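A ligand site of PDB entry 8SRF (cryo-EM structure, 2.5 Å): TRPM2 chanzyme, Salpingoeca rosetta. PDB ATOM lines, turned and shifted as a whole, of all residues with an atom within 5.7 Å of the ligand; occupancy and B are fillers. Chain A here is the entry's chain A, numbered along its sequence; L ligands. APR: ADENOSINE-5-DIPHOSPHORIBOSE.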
ATOM      1  N   VAL A 147      -1.960  27.685  -8.105  1.00  0.00           N
ATOM      2  CA  VAL A 147      -2.307  28.127  -6.754  1.00  0.00           C
ATOM      3  C   VAL A 147      -2.929  26.945  -6.022  1.00  0.00           C
ATOM      4  O   VAL A 147      -3.994  26.464  -6.417  1.00  0.00           O
ATOM      5  CB  VAL A 147      -3.230  29.355  -6.757  1.00  0.00           C
ATOM      6  CG1 VAL A 147      -3.348  29.898  -5.347  1.00  0.00           C
ATOM      7  CG2 VAL A 147      -2.641  30.430  -7.638  1.00  0.00           C
ATOM      8  N   THR A 148      -2.265  26.485  -4.965  1.00  0.00           N
ATOM      9  CA  THR A 148      -2.778  25.389  -4.151  1.00  0.00           C
ATOM     10  C   THR A 148      -2.853  25.769  -2.684  1.00  0.00           C
ATOM     11  O   THR A 148      -2.239  26.746  -2.239  1.00  0.00           O
ATOM     12  CB  THR A 148      -1.910  24.136  -4.312  1.00  0.00           C
ATOM     13  OG1 THR A 148      -2.390  23.107  -3.457  1.00  0.00           O
ATOM     14  CG2 THR A 148      -0.450  24.437  -3.968  1.00  0.00           C
ATOM     15  N   GLY A 149      -3.634  25.000  -1.933  1.00  0.00           N
ATOM     16  CA  GLY A 149      -3.714  25.230  -0.497  1.00  0.00           C
ATOM     17  C   GLY A 149      -5.019  24.777   0.136  1.00  0.00           C
ATOM     18  O   GLY A 149      -5.620  23.778  -0.271  1.00  0.00           O
ATOM     19  N   GLY A 150      -5.354  25.508   1.200  1.00  0.00           N
ATOM     20  CA  GLY A 150      -6.491  25.179   2.056  1.00  0.00           C
ATOM     21  C   GLY A 150      -7.829  25.370   1.376  1.00  0.00           C
ATOM     22  O   GLY A 150      -8.054  26.396   0.719  1.00  0.00           O
ATOM     23  N   ALA A 151      -8.701  24.350   1.438  1.00  0.00           N
ATOM     24  CA  ALA A 151     -10.037  24.589   0.903  1.00  0.00           C
ATOM     25  C   ALA A 151     -11.155  24.656   1.929  1.00  0.00           C
ATOM     26  O   ALA A 151     -11.919  25.622   1.896  1.00  0.00           O
ATOM     27  CB  ALA A 151     -10.326  23.452  -0.067  1.00  0.00           C
ATOM     28  N   ARG A 152     -11.246  23.719   2.888  1.00  0.00           N
ATOM     29  CA  ARG A 152     -12.315  23.820   3.882  1.00  0.00           C
ATOM     30  C   ARG A 152     -12.013  24.824   4.984  1.00  0.00           C
ATOM     31  O   ARG A 152     -12.633  25.877   5.048  1.00  0.00           O
ATOM     32  CB  ARG A 152     -12.669  22.448   4.468  1.00  0.00           C
ATOM     33  CG  ARG A 152     -13.576  21.723   3.483  1.00  0.00           C
ATOM     34  CD  ARG A 152     -14.651  20.840   4.129  1.00  0.00           C
ATOM     35  NE  ARG A 152     -15.569  20.232   3.155  1.00  0.00           N
ATOM     36  CZ  ARG A 152     -16.577  20.824   2.526  1.00  0.00           C
ATOM     37  NH1 ARG A 152     -16.894  22.099   2.736  1.00  0.00           N
ATOM     38  NH2 ARG A 152     -17.306  20.118   1.662  1.00  0.00           N
ATOM     39  N   ASN A 153     -11.034  24.480   5.844  1.00  0.00           N
ATOM     40  CA  ASN A 153     -10.501  25.212   6.986  1.00  0.00           C
ATOM     41  C   ASN A 153      -9.450  26.179   6.373  1.00  0.00           C
ATOM     42  O   ASN A 153      -8.251  25.937   6.575  1.00  0.00           O
ATOM     43  CB  ASN A 153      -9.647  24.265   7.844  1.00  0.00           C
ATOM     44  CG  ASN A 153      -8.455  23.672   7.082  1.00  0.00           C
ATOM     45  OD1 ASN A 153      -8.386  23.730   5.860  1.00  0.00           O
ATOM     46  ND2 ASN A 153      -7.527  23.089   7.826  1.00  0.00           N
ATOM     47  N   PHE A 154      -9.931  27.081   5.515  1.00  0.00           N
ATOM     48  CA  PHE A 154      -9.070  28.159   4.968  1.00  0.00           C
ATOM     49  C   PHE A 154      -9.667  29.453   5.506  1.00  0.00           C
ATOM     50  O   PHE A 154     -10.542  30.030   4.854  1.00  0.00           O
ATOM     51  CB  PHE A 154      -9.083  28.235   3.440  1.00  0.00           C
ATOM     52  CG  PHE A 154      -8.193  29.308   2.878  1.00  0.00           C
ATOM     53  CD1 PHE A 154      -6.812  29.183   2.948  1.00  0.00           C
ATOM     54  CD2 PHE A 154      -8.724  30.456   2.312  1.00  0.00           C
ATOM     55  CE1 PHE A 154      -5.989  30.176   2.448  1.00  0.00           C
ATOM     56  CE2 PHE A 154      -7.891  31.447   1.820  1.00  0.00           C
ATOM     57  CZ  PHE A 154      -6.535  31.305   1.886  1.00  0.00           C
ATOM     58  N   GLY A 182      -7.472  24.094  -8.044  1.00  0.00           N
ATOM     59  CA  GLY A 182      -8.432  23.023  -8.028  1.00  0.00           C
ATOM     60  C   GLY A 182      -9.727  23.503  -8.656  1.00  0.00           C
ATOM     61  O   GLY A 182     -10.019  24.699  -8.757  1.00  0.00           O
ATOM     62  N   THR A 184     -12.786  23.108  -7.291  1.00  0.00           N
ATOM     63  CA  THR A 184     -13.895  23.349  -6.374  1.00  0.00           C
ATOM     64  C   THR A 184     -14.055  24.781  -5.853  1.00  0.00           C
ATOM     65  O   THR A 184     -13.149  25.608  -5.923  1.00  0.00           O
ATOM     66  CB  THR A 184     -13.747  22.395  -5.192  1.00  0.00           C
ATOM     67  OG1 THR A 184     -12.635  22.802  -4.396  1.00  0.00           O
ATOM     68  CG2 THR A 184     -13.481  20.969  -5.696  1.00  0.00           C
ATOM     69  N   THR A 186     -14.230  26.367  -2.988  1.00  0.00           N
ATOM     70  CA  THR A 186     -13.822  26.524  -1.600  1.00  0.00           C
ATOM     71  C   THR A 186     -12.423  27.107  -1.511  1.00  0.00           C
ATOM     72  O   THR A 186     -11.573  26.844  -2.368  1.00  0.00           O
ATOM     73  CB  THR A 186     -13.841  25.168  -0.851  1.00  0.00           C
ATOM     74  OG1 THR A 186     -13.222  24.156  -1.656  1.00  0.00           O
ATOM     75  CG2 THR A 186     -15.211  24.723  -0.294  1.00  0.00           C
ATOM     76  N   VAL A 188      -8.847  29.039  -1.009  1.00  0.00           N
ATOM     77  CA  VAL A 188      -7.874  29.842  -1.758  1.00  0.00           C
ATOM     78  C   VAL A 188      -8.121  29.741  -3.272  1.00  0.00           C
ATOM     79  O   VAL A 188      -7.840  30.683  -4.012  1.00  0.00           O
ATOM     80  CB  VAL A 188      -6.422  29.497  -1.296  1.00  0.00           C
ATOM     81  CG1 VAL A 188      -5.896  28.110  -1.723  1.00  0.00           C
ATOM     82  CG2 VAL A 188      -5.419  30.601  -1.651  1.00  0.00           C
ATOM     83  N   MET A 189      -8.629  28.582  -3.735  1.00  0.00           N
ATOM     84  CA  MET A 189      -9.012  28.356  -5.131  1.00  0.00           C
ATOM     85  C   MET A 189     -10.190  29.233  -5.528  1.00  0.00           C
ATOM     86  O   MET A 189     -10.225  29.770  -6.649  1.00  0.00           O
ATOM     87  CB  MET A 189      -9.260  26.870  -5.346  1.00  0.00           C
ATOM     88  CG  MET A 189      -8.019  26.114  -4.894  1.00  0.00           C
ATOM     89  SD  MET A 189      -8.163  24.363  -4.585  1.00  0.00           S
ATOM     90  CE  MET A 189      -9.684  24.353  -3.690  1.00  0.00           C
ATOM     91  N   ILE A 213      -8.341  21.437 -11.755  1.00  0.00           N
ATOM     92  CA  ILE A 213      -8.105  20.011 -11.725  1.00  0.00           C
ATOM     93  C   ILE A 213      -8.613  19.467 -10.396  1.00  0.00           C
ATOM     94  O   ILE A 213      -8.060  19.785  -9.340  1.00  0.00           O
ATOM     95  CB  ILE A 213      -6.616  19.690 -11.897  1.00  0.00           C
ATOM     96  CG1 ILE A 213      -6.075  20.344 -13.181  1.00  0.00           C
ATOM     97  CG2 ILE A 213      -6.392  18.187 -11.853  1.00  0.00           C
ATOM     98  CD1 ILE A 213      -4.623  20.055 -13.437  1.00  0.00           C
ATOM     99  N   THR A 248     -19.249  18.627  -2.298  1.00  0.00           N
ATOM    100  CA  THR A 248     -18.338  19.679  -2.740  1.00  0.00           C
ATOM    101  C   THR A 248     -18.653  20.178  -4.157  1.00  0.00           C
ATOM    102  O   THR A 248     -18.485  19.413  -5.115  1.00  0.00           O
ATOM    103  CB  THR A 248     -16.908  19.167  -2.649  1.00  0.00           C
ATOM    104  OG1 THR A 248     -16.642  18.780  -1.300  1.00  0.00           O
ATOM    105  CG2 THR A 248     -15.993  20.288  -2.934  1.00  0.00           C
ATOM    106  N   PHE A 268     -10.246  12.423  -1.401  1.00  0.00           N
ATOM    107  CA  PHE A 268      -9.515  13.581  -1.882  1.00  0.00           C
ATOM    108  C   PHE A 268      -8.043  13.246  -2.103  1.00  0.00           C
ATOM    109  O   PHE A 268      -7.536  12.205  -1.661  1.00  0.00           O
ATOM    110  CB  PHE A 268      -9.655  14.751  -0.901  1.00  0.00           C
ATOM    111  CG  PHE A 268     -11.044  15.312  -0.816  1.00  0.00           C
ATOM    112  CD1 PHE A 268     -11.457  16.294  -1.735  1.00  0.00           C
ATOM    113  CD2 PHE A 268     -11.944  14.855   0.164  1.00  0.00           C
ATOM    114  CE1 PHE A 268     -12.743  16.838  -1.670  1.00  0.00           C
ATOM    115  CE2 PHE A 268     -13.249  15.395   0.241  1.00  0.00           C
ATOM    116  CZ  PHE A 268     -13.644  16.374  -0.678  1.00  0.00           C
ATOM    117  N   GLY A 269      -7.363  14.134  -2.797  1.00  0.00           N
ATOM    118  CA  GLY A 269      -5.941  14.029  -3.041  1.00  0.00           C
ATOM    119  C   GLY A 269      -5.506  13.073  -4.121  1.00  0.00           C
ATOM    120  O   GLY A 269      -4.320  12.774  -4.224  1.00  0.00           O
ATOM    121  N   GLU A 271      -5.766  13.629  -7.365  1.00  0.00           N
ATOM    122  CA  GLU A 271      -5.439  14.355  -8.582  1.00  0.00           C
ATOM    123  C   GLU A 271      -4.080  15.051  -8.527  1.00  0.00           C
ATOM    124  O   GLU A 271      -3.693  15.659  -9.541  1.00  0.00           O
ATOM    125  CB  GLU A 271      -6.539  15.396  -8.843  1.00  0.00           C
ATOM    126  CG  GLU A 271      -6.488  16.752  -8.062  1.00  0.00           C
ATOM    127  CD  GLU A 271      -6.967  16.752  -6.629  1.00  0.00           C
ATOM    128  OE1 GLU A 271      -7.311  15.692  -6.071  1.00  0.00           O
ATOM    129  OE2 GLU A 271      -7.037  17.848  -6.039  1.00  0.00           O
ATOM    130  N   ILE A 272      -3.349  14.883  -7.414  1.00  0.00           N
ATOM    131  CA  ILE A 272      -2.083  15.580  -7.089  1.00  0.00           C
ATOM    132  C   ILE A 272      -0.937  15.260  -8.067  1.00  0.00           C
ATOM    133  O   ILE A 272      -0.276  16.199  -8.567  1.00  0.00           O
ATOM    134  CB  ILE A 272      -1.713  15.259  -5.619  1.00  0.00           C
ATOM    135  CG1 ILE A 272      -2.732  15.797  -4.615  1.00  0.00           C
ATOM    136  CG2 ILE A 272      -0.291  15.546  -5.265  1.00  0.00           C
ATOM    137  CD1 ILE A 272      -2.444  15.396  -3.158  1.00  0.00           C
ATOM    138  N   ARG A 275      -1.767  16.551 -11.553  1.00  0.00           N
ATOM    139  CA  ARG A 275      -1.675  18.026 -11.555  1.00  0.00           C
ATOM    140  C   ARG A 275      -0.231  18.493 -11.705  1.00  0.00           C
ATOM    141  O   ARG A 275       0.032  19.371 -12.538  1.00  0.00           O
ATOM    142  CB  ARG A 275      -2.316  18.618 -10.298  1.00  0.00           C
ATOM    143  CG  ARG A 275      -2.325  20.126 -10.257  1.00  0.00           C
ATOM    144  CD  ARG A 275      -2.951  20.666  -8.993  1.00  0.00           C
ATOM    145  NE  ARG A 275      -2.560  22.058  -8.768  1.00  0.00           N
ATOM    146  CZ  ARG A 275      -3.097  22.845  -7.853  1.00  0.00           C
ATOM    147  NH1 ARG A 275      -4.065  22.422  -7.057  1.00  0.00           N
ATOM    148  NH2 ARG A 275      -2.670  24.099  -7.745  1.00  0.00           N
ATOM    149  N   GLY A 297      -3.058  25.459   3.739  1.00  0.00           N
ATOM    150  CA  GLY A 297      -3.014  24.091   3.285  1.00  0.00           C
ATOM    151  C   GLY A 297      -3.031  23.032   4.383  1.00  0.00           C
ATOM    152  O   GLY A 297      -2.699  23.274   5.547  1.00  0.00           O
ATOM    153  N   GLY A 298      -3.544  21.883   3.964  1.00  0.00           N
ATOM    154  CA  GLY A 298      -3.642  20.662   4.734  1.00  0.00           C
ATOM    155  C   GLY A 298      -2.613  19.638   4.256  1.00  0.00           C
ATOM    156  O   GLY A 298      -1.564  20.020   3.730  1.00  0.00           O
ATOM    157  N   PRO A 299      -2.833  18.329   4.579  1.00  0.00           N
ATOM    158  CA  PRO A 299      -1.918  17.252   4.123  1.00  0.00           C
ATOM    159  C   PRO A 299      -1.752  17.064   2.607  1.00  0.00           C
ATOM    160  O   PRO A 299      -0.665  16.669   2.153  1.00  0.00           O
ATOM    161  CB  PRO A 299      -2.525  15.993   4.752  1.00  0.00           C
ATOM    162  CG  PRO A 299      -3.331  16.465   5.876  1.00  0.00           C
ATOM    163  CD  PRO A 299      -3.876  17.800   5.486  1.00  0.00           C
ATOM    164  N   GLY A 300      -2.821  17.303   1.833  1.00  0.00           N
ATOM    165  CA  GLY A 300      -2.715  17.162   0.391  1.00  0.00           C
ATOM    166  C   GLY A 300      -1.929  18.284  -0.271  1.00  0.00           C
ATOM    167  O   GLY A 300      -1.412  18.103  -1.368  1.00  0.00           O
ATOM    168  N   THR A 301      -1.900  19.467   0.369  1.00  0.00           N
ATOM    169  CA  THR A 301      -1.077  20.582  -0.099  1.00  0.00           C
ATOM    170  C   THR A 301       0.411  20.264   0.044  1.00  0.00           C
ATOM    171  O   THR A 301       1.235  20.650  -0.806  1.00  0.00           O
ATOM    172  CB  THR A 301      -1.517  21.802   0.709  1.00  0.00           C
ATOM    173  OG1 THR A 301      -2.879  22.087   0.364  1.00  0.00           O
ATOM    174  CG2 THR A 301      -0.727  23.057   0.423  1.00  0.00           C
ATOM    175  N   THR A 304       1.084  17.936  -2.697  1.00  0.00           N
ATOM    176  CA  THR A 304       1.151  18.761  -3.911  1.00  0.00           C
ATOM    177  C   THR A 304       2.524  19.411  -4.079  1.00  0.00           C
ATOM    178  O   THR A 304       3.109  19.355  -5.183  1.00  0.00           O
ATOM    179  CB  THR A 304       0.021  19.809  -3.867  1.00  0.00           C
ATOM    180  OG1 THR A 304      -1.248  19.136  -3.907  1.00  0.00           O
ATOM    181  CG2 THR A 304       0.063  20.783  -5.046  1.00  0.00           C
HETATM  182  N1  APR L   1     -11.917  20.938  -2.414  1.00  0.00           N
HETATM  183  C2  APR L   1     -12.806  20.967  -1.410  1.00  0.00           C
HETATM  184  N3  APR L   1     -12.614  20.358  -0.235  1.00  0.00           N
HETATM  185  C4  APR L   1     -11.492  19.670  -0.011  1.00  0.00           C
HETATM  186  C5  APR L   1     -10.470  19.590  -1.056  1.00  0.00           C
HETATM  187  C6  APR L   1     -10.754  20.290  -2.316  1.00  0.00           C
HETATM  188  N6  APR L   1      -9.865  20.267  -3.332  1.00  0.00           N
HETATM  189  N7  APR L   1      -9.468  18.851  -0.561  1.00  0.00           N
HETATM  190  C8  APR L   1      -9.815  18.487   0.699  1.00  0.00           C
HETATM  191  N9  APR L   1     -11.021  18.976   1.010  1.00  0.00           N
HETATM  192  C1' APR L   1     -11.749  18.802   2.281  1.00  0.00           C
HETATM  193  C2' APR L   1     -11.584  17.387   2.773  1.00  0.00           C
HETATM  194  O2' APR L   1     -12.869  16.916   3.159  1.00  0.00           O
HETATM  195  C3' APR L   1     -10.703  17.457   3.990  1.00  0.00           C
HETATM  196  O3' APR L   1     -11.211  16.595   5.000  1.00  0.00           O
HETATM  197  O4' APR L   1     -11.179  19.652   3.280  1.00  0.00           O
HETATM  198  C4' APR L   1     -10.811  18.899   4.435  1.00  0.00           C
HETATM  199  C5' APR L   1      -9.489  19.442   4.927  1.00  0.00           C
HETATM  200  O5' APR L   1      -9.339  20.702   4.305  1.00  0.00           O
HETATM  201  PA  APR L   1      -7.890  21.180   3.816  1.00  0.00           P
HETATM  202  O1A APR L   1      -8.077  22.554   3.275  1.00  0.00           O
HETATM  203  O2A APR L   1      -6.933  20.927   4.937  1.00  0.00           O
HETATM  204  O3A APR L   1      -7.539  20.177   2.628  1.00  0.00           O
HETATM  205  PB  APR L   1      -6.162  20.385   1.859  1.00  0.00           P
HETATM  206  O1B APR L   1      -5.285  19.185   2.089  1.00  0.00           O
HETATM  207  O2B APR L   1      -5.657  21.767   2.109  1.00  0.00           O
HETATM  208  O5D APR L   1      -6.578  20.361   0.332  1.00  0.00           O
HETATM  209  C5D APR L   1      -5.700  19.706  -0.559  1.00  0.00           C
HETATM  210  O4D APR L   1      -6.347  21.460  -2.027  1.00  0.00           O
HETATM  211  O1D APR L   1      -5.354  23.200  -3.182  1.00  0.00           O
HETATM  212  C1D APR L   1      -5.938  21.914  -3.304  1.00  0.00           C
HETATM  213  O2D APR L   1      -5.230  20.575  -5.168  1.00  0.00           O
HETATM  214  C2D APR L   1      -4.918  20.926  -3.820  1.00  0.00           C
HETATM  215  O3D APR L   1      -5.547  18.620  -3.783  1.00  0.00           O
HETATM  216  C3D APR L   1      -5.080  19.697  -2.959  1.00  0.00           C
HETATM  217  C4D APR L   1      -6.145  20.055  -1.950  1.00  0.00           C
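The backbone NH (N) of Ala 151 lies within hydrogen-bond range of an oxygen (O1A) of the ligand, at 2.6 Å.
N of Gly 149 is in hydrogen-bond range of O1D of the ligand (2.8 Å).
The backbone carbonyl oxygen (O) of Gly 149 lies within hydrogen-bond range of an oxygen (O1D) of the ligand (3.0 Å).
The side-chain carboxylate of Glu 271 lies within hydrogen-bond range of an oxygen (O3D) of the ligand, at 2.8 Å.
An oxygen (O2B) of the ligand lies within hydrogen-bond range of the backbone NH of Gly 298.
OG1 of Thr 184 lies within hydrogen-bond range of N1 of the ligand, at 2.8 Å.
OD1 of Asn 153 lies close to O1A of the ligand (2.9 Å).
An oxygen (O2D) of the ligand is in hydrogen-bond range of the guanidinium group (NH1) of Arg 275, 2.9 Å away.
OG1 of Thr 148 sits at hydrogen-bond distance from O1D of the ligand, at 3.0 Å.
N of Gly 300 lies within hydrogen-bond range of O1B of the ligand, at 3.1 Å.
O1A of the ligand is in hydrogen-bond range of N of Arg 152, at 3.4 Å.
An oxygen (O2B) of the ligand lies within hydrogen-bond range of the side-chain hydroxyl (OG1) of Thr 301, at 3.3 Å.
The side-chain sulfur (SD) of Met 189 lies within hydrogen-bond range of an oxygen (O1D) of the ligand, at 3.3 Å.
Residues that only touch the ligand: Thr 186, Gly 150, Phe 268, Thr 248, Pro 299, Gly 297 and Thr 304.
Hydrophobic or aromatic side chains that line the ligand: Ala 151, Met 189, Phe 268 and Pro 299.
19 residues have an atom within 4 Å of the ligand: Thr 148, Gly 149, Gly 150, Ala 151, Arg 152, Asn 153, Thr 184, Thr 186, Met 189, Thr 248, Phe 268, Glu 271, Arg 275, Gly 297, Gly 298, Pro 299, Gly 300, Thr 301 and Thr 304.
The nearest printed residue that does not touch the ligand is Ile 272 (4.1 Å).
The backbone carbonyl oxygen (O) of Gly 149 lies within hydrogen-bond range of the side-chain hydroxyl (OG1) of Thr 301 (3.3 Å).
OG1 of Thr 184 lies within hydrogen-bond range of OG1 of Thr 186 (3.1 Å).
The guanidinium group (NH2) of Arg 275 sits at hydrogen-bond distance from the backbone carbonyl oxygen (O) of Val 147 (3.0 Å).
The backbone carbonyl oxygen (O) of Gly 300 is in hydrogen-bond range of the side-chain hydroxyl (OG1) of Thr 304, 2.7 Å away.
OG1 of Thr 248 sits at hydrogen-bond distance from NH2 of Arg 152, at 3.3 Å.
N of Val 188 sits at hydrogen-bond distance from O of Gly 150, at 3.3 Å.
SD of Met 189 sits at hydrogen-bond distance from N of Gly 182.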
